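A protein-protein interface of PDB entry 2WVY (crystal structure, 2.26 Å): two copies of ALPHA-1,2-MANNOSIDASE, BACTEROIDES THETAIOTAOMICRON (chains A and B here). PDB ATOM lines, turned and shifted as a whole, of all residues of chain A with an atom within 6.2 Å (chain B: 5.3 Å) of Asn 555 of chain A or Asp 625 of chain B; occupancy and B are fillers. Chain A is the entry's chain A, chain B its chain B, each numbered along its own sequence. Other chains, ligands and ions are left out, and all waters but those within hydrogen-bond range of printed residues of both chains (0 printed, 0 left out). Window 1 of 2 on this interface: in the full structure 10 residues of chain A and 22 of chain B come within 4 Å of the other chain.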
ATOM      1  N   ALA A 553      -1.905  17.814  -2.854  1.00  0.00           N
ATOM      2  CA  ALA A 553      -1.633  17.077  -1.637  1.00  0.00           C
ATOM      3  C   ALA A 553      -2.908  16.429  -1.184  1.00  0.00           C
ATOM      4  O   ALA A 553      -3.993  16.850  -1.581  1.00  0.00           O
ATOM      5  CB  ALA A 553      -1.118  17.996  -0.554  1.00  0.00           C
ATOM      6  N   PRO A 554      -2.782  15.402  -0.342  1.00  0.00           N
ATOM      7  CA  PRO A 554      -4.023  14.829   0.148  1.00  0.00           C
ATOM      8  C   PRO A 554      -4.775  15.821   1.048  1.00  0.00           C
ATOM      9  O   PRO A 554      -4.172  16.465   1.907  1.00  0.00           O
ATOM     10  CB  PRO A 554      -3.540  13.630   0.964  1.00  0.00           C
ATOM     11  N   ASN A 555      -6.079  15.960   0.829  1.00  0.00           N
ATOM     12  CA  ASN A 555      -6.933  16.687   1.767  1.00  0.00           C
ATOM     13  C   ASN A 555      -7.850  15.712   2.501  1.00  0.00           C
ATOM     14  O   ASN A 555      -8.748  15.135   1.909  1.00  0.00           O
ATOM     15  CB  ASN A 555      -7.764  17.738   1.043  1.00  0.00           C
ATOM     16  CG  ASN A 555      -8.480  18.677   2.003  1.00  0.00           C
ATOM     17  OD1 ASN A 555      -8.535  18.428   3.207  1.00  0.00           O
ATOM     18  ND2 ASN A 555      -9.040  19.756   1.471  1.00  0.00           N
ATOM     19  N   THR A 556      -7.611  15.529   3.796  1.00  0.00           N
ATOM     20  CA  THR A 556      -8.393  14.601   4.594  1.00  0.00           C
ATOM     21  C   THR A 556      -9.503  15.288   5.355  1.00  0.00           C
ATOM     22  O   THR A 556     -10.355  14.619   5.927  1.00  0.00           O
ATOM     23  CB  THR A 556      -7.525  13.952   5.665  1.00  0.00           C
ATOM     24  OG1 THR A 556      -6.711  14.964   6.267  1.00  0.00           O
ATOM     25  CG2 THR A 556      -6.614  12.891   5.054  1.00  0.00           C
ATOM     26  N   TYR A 557      -9.460  16.614   5.405  1.00  0.00           N
ATOM     27  CA  TYR A 557     -10.420  17.368   6.191  1.00  0.00           C
ATOM     28  C   TYR A 557     -10.358  16.909   7.639  1.00  0.00           C
ATOM     29  O   TYR A 557      -9.279  16.748   8.200  1.00  0.00           O
ATOM     30  CB  TYR A 557     -11.826  17.163   5.638  1.00  0.00           C
ATOM     31  CG  TYR A 557     -11.903  17.438   4.161  1.00  0.00           C
ATOM     32  CD1 TYR A 557     -12.242  18.692   3.697  1.00  0.00           C
ATOM     33  CD2 TYR A 557     -11.604  16.451   3.230  1.00  0.00           C
ATOM     34  CE1 TYR A 557     -12.306  18.966   2.351  1.00  0.00           C
ATOM     35  CE2 TYR A 557     -11.670  16.706   1.872  1.00  0.00           C
ATOM     36  CZ  TYR A 557     -12.021  17.974   1.436  1.00  0.00           C
ATOM     37  OH  TYR A 557     -12.086  18.271   0.089  1.00  0.00           O
ATOM     38  N   ASN A 558     -11.524  16.675   8.230  1.00  0.00           N
ATOM     39  CA  ASN A 558     -11.607  16.201   9.609  1.00  0.00           C
ATOM     40  C   ASN A 558     -11.698  14.673   9.705  1.00  0.00           C
ATOM     41  O   ASN A 558     -11.975  14.124  10.772  1.00  0.00           O
ATOM     42  CB  ASN A 558     -12.802  16.849  10.323  1.00  0.00           C
ATOM     43  CG  ASN A 558     -12.652  18.354  10.475  1.00  0.00           C
ATOM     44  OD1 ASN A 558     -11.542  18.872  10.563  1.00  0.00           O
ATOM     45  ND2 ASN A 558     -13.774  19.062  10.517  1.00  0.00           N
ATOM     46  N   ALA A 570      -6.679   8.827   0.903  1.00  0.00           N
ATOM     47  CA  ALA A 570      -6.726  10.192   0.404  1.00  0.00           C
ATOM     48  C   ALA A 570      -5.663  10.453  -0.665  1.00  0.00           C
ATOM     49  O   ALA A 570      -5.911  11.148  -1.646  1.00  0.00           O
ATOM     50  CB  ALA A 570      -6.577  11.172   1.548  1.00  0.00           C
ATOM     51  N   ALA A 574      -5.832  11.859  -4.689  1.00  0.00           N
ATOM     52  CA  ALA A 574      -5.101  13.058  -5.092  1.00  0.00           C
ATOM     53  C   ALA A 574      -4.211  12.778  -6.304  1.00  0.00           C
ATOM     54  O   ALA A 574      -4.018  13.641  -7.172  1.00  0.00           O
ATOM     55  CB  ALA A 574      -4.269  13.579  -3.934  1.00  0.00           C
ATOM     56  N   MET B 572     -15.299  11.989   1.757  1.00  0.00           N
ATOM     57  CA  MET B 572     -14.085  12.718   1.381  1.00  0.00           C
ATOM     58  C   MET B 572     -14.078  12.948  -0.106  1.00  0.00           C
ATOM     59  O   MET B 572     -13.842  14.058  -0.576  1.00  0.00           O
ATOM     60  CB  MET B 572     -12.833  11.916   1.683  1.00  0.00           C
ATOM     61  CG  MET B 572     -12.346  11.955   3.087  1.00  0.00           C
ATOM     62  SD  MET B 572     -10.625  11.424   3.092  1.00  0.00           S
ATOM     63  CE  MET B 572     -10.651  10.220   4.421  1.00  0.00           C
ATOM     64  N   LEU B 575     -16.358  15.778  -1.502  1.00  0.00           N
ATOM     65  CA  LEU B 575     -15.755  17.047  -1.126  1.00  0.00           C
ATOM     66  C   LEU B 575     -14.522  17.304  -1.990  1.00  0.00           C
ATOM     67  O   LEU B 575     -14.355  18.394  -2.549  1.00  0.00           O
ATOM     68  CB  LEU B 575     -15.381  17.031   0.355  1.00  0.00           C
ATOM     69  CG  LEU B 575     -16.599  16.909   1.264  1.00  0.00           C
ATOM     70  CD1 LEU B 575     -16.181  16.745   2.714  1.00  0.00           C
ATOM     71  CD2 LEU B 575     -17.474  18.133   1.083  1.00  0.00           C
ATOM     72  N   ASN B 576     -13.650  16.301  -2.077  1.00  0.00           N
ATOM     73  CA  ASN B 576     -12.475  16.408  -2.921  1.00  0.00           C
ATOM     74  C   ASN B 576     -13.000  16.787  -4.283  1.00  0.00           C
ATOM     75  O   ASN B 576     -12.353  17.509  -5.044  1.00  0.00           O
ATOM     76  CB  ASN B 576     -11.724  15.080  -2.993  1.00  0.00           C
ATOM     77  CG  ASN B 576     -10.773  14.878  -1.825  1.00  0.00           C
ATOM     78  OD1 ASN B 576     -10.173  15.828  -1.317  1.00  0.00           O
ATOM     79  ND2 ASN B 576     -10.625  13.632  -1.398  1.00  0.00           N
ATOM     80  N   CYS B 623     -10.770  24.055   5.848  1.00  0.00           N
ATOM     81  CA  CYS B 623     -10.438  22.869   5.025  1.00  0.00           C
ATOM     82  C   CYS B 623     -11.019  22.946   3.633  1.00  0.00           C
ATOM     83  O   CYS B 623     -10.640  22.171   2.761  1.00  0.00           O
ATOM     84  CB  CYS B 623     -10.971  21.557   5.641  1.00  0.00           C
ATOM     85  SG  CYS B 623     -10.669  21.276   7.388  1.00  0.00           S
ATOM     86  N   GLY B 624     -11.987  23.831   3.436  1.00  0.00           N
ATOM     87  CA  GLY B 624     -12.605  23.964   2.129  1.00  0.00           C
ATOM     88  C   GLY B 624     -11.524  24.324   1.132  1.00  0.00           C
ATOM     89  O   GLY B 624     -10.728  25.231   1.373  1.00  0.00           O
ATOM     90  N   ASP B 625     -11.480  23.612   0.015  1.00  0.00           N
ATOM     91  CA  ASP B 625     -10.420  23.831  -0.960  1.00  0.00           C
ATOM     92  C   ASP B 625     -10.392  25.269  -1.462  1.00  0.00           C
ATOM     93  O   ASP B 625      -9.327  25.807  -1.747  1.00  0.00           O
ATOM     94  CB  ASP B 625     -10.543  22.844  -2.126  1.00  0.00           C
ATOM     95  CG  ASP B 625     -10.029  21.448  -1.768  1.00  0.00           C
ATOM     96  OD1 ASP B 625      -9.294  21.326  -0.755  1.00  0.00           O
ATOM     97  OD2 ASP B 625     -10.350  20.481  -2.499  1.00  0.00           O
ATOM     98  N   GLU B 626     -11.566  25.883  -1.563  1.00  0.00           N
ATOM     99  CA  GLU B 626     -11.677  27.270  -2.004  1.00  0.00           C
ATOM    100  C   GLU B 626     -11.815  28.222  -0.826  1.00  0.00           C
ATOM    101  O   GLU B 626     -12.178  29.382  -1.003  1.00  0.00           O
ATOM    102  CB  GLU B 626     -12.888  27.445  -2.925  1.00  0.00           C
ATOM    103  CG  GLU B 626     -12.762  26.777  -4.289  1.00  0.00           C
ATOM    104  CD  GLU B 626     -13.953  27.081  -5.196  1.00  0.00           C
ATOM    105  OE1 GLU B 626     -15.085  26.642  -4.885  1.00  0.00           O
ATOM    106  OE2 GLU B 626     -13.756  27.763  -6.224  1.00  0.00           O
ATOM    107  N   ASP B 627     -11.534  27.730   0.376  1.00  0.00           N
ATOM    108  CA  ASP B 627     -11.739  28.520   1.594  1.00  0.00           C
ATOM    109  C   ASP B 627     -10.388  28.890   2.227  1.00  0.00           C
ATOM    110  O   ASP B 627      -9.694  28.034   2.781  1.00  0.00           O
ATOM    111  CB  ASP B 627     -12.639  27.743   2.572  1.00  0.00           C
ATOM    112  CG  ASP B 627     -13.078  28.565   3.793  1.00  0.00           C
ATOM    113  OD1 ASP B 627     -12.957  29.821   3.805  1.00  0.00           O
ATOM    114  OD2 ASP B 627     -13.566  27.923   4.754  1.00  0.00           O
ATOM    115  N   ASN B 628     -10.013  30.161   2.128  1.00  0.00           N
ATOM    116  CA  ASN B 628      -8.778  30.638   2.753  1.00  0.00           C
ATOM    117  C   ASN B 628      -9.012  31.551   3.951  1.00  0.00           C
ATOM    118  O   ASN B 628      -8.105  32.281   4.360  1.00  0.00           O
ATOM    119  CB  ASN B 628      -7.898  31.368   1.735  1.00  0.00           C
ATOM    120  CG  ASN B 628      -7.746  30.596   0.445  1.00  0.00           C
ATOM    121  OD1 ASN B 628      -8.255  31.006  -0.597  1.00  0.00           O
ATOM    122  ND2 ASN B 628      -7.063  29.457   0.512  1.00  0.00           N
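Of the printed residues of chain B, Asn 555 of chain A touches Asn 576, Cys 623 and Asp 625. Of the printed residues of chain A, Cys 623 of chain B touches Asn 555 and Tyr 557. Printed residues of chain A within 4 Å of Leu 575 of chain B: Tyr 557. Of the printed residues of chain A, Asn 576 of chain B touches Asn 555 and Tyr 557. Of the printed residues of chain B, Tyr 557 of chain A touches Leu 575, Asn 576, Cys 623 and Asp 625. Ala 570 of chain A touches none of the printed residues of chain B. The nearest printed residue of chain A that does not touch Asp 625 of chain B is Ala 553 of chain A (7.0 Å).
Among the printed residues, merely in contact across the chains: Asn 555 of chain A with Asn 576 of chain B, Tyr 557 of chain A with Cys 623 of chain B and Tyr 557 of chain A with Asp 625 of chain B.
The backbone NH (N) of Tyr 557 of chain A lies within hydrogen-bond range of the side-chain amide oxygen (OD1) of Asn 555 of chain A (3.0 Å). O of Met 572 of chain B sits at hydrogen-bond distance from ND2 of Asn 576 of chain B.
Printed residues of chain A that touch a printed residue of chain B: Asn 555 and Tyr 557. Hydrophobic or aromatic side chains of chain A within 4 Å of the printed part of chain B: Tyr 557. Among the printed residues, no Asp or Glu carboxylate lies within 4 Å of a Lys or Arg side-chain nitrogen of the other chain.
No position is printed for both chains. Of the 7 pairs that touch across the chains among the printed residues, none has its exchanged pair printed and touching as well.
OH of Tyr 557 of chain A is in hydrogen-bond range of N of Asn 576 of chain B (3.3 Å). ND2 of Asn 555 of chain A lies within hydrogen-bond range of O of Cys 623 of chain B, at 3.2 Å. ND2 of Asn 555 of chain A lies within hydrogen-bond range of OD1 of Asp 625 of chain B, 2.7 Å away. The side-chain hydroxyl (OH) of Tyr 557 of chain A sits close to the backbone carbonyl oxygen (O) of Leu 575 of chain B, at 3.5 Å.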
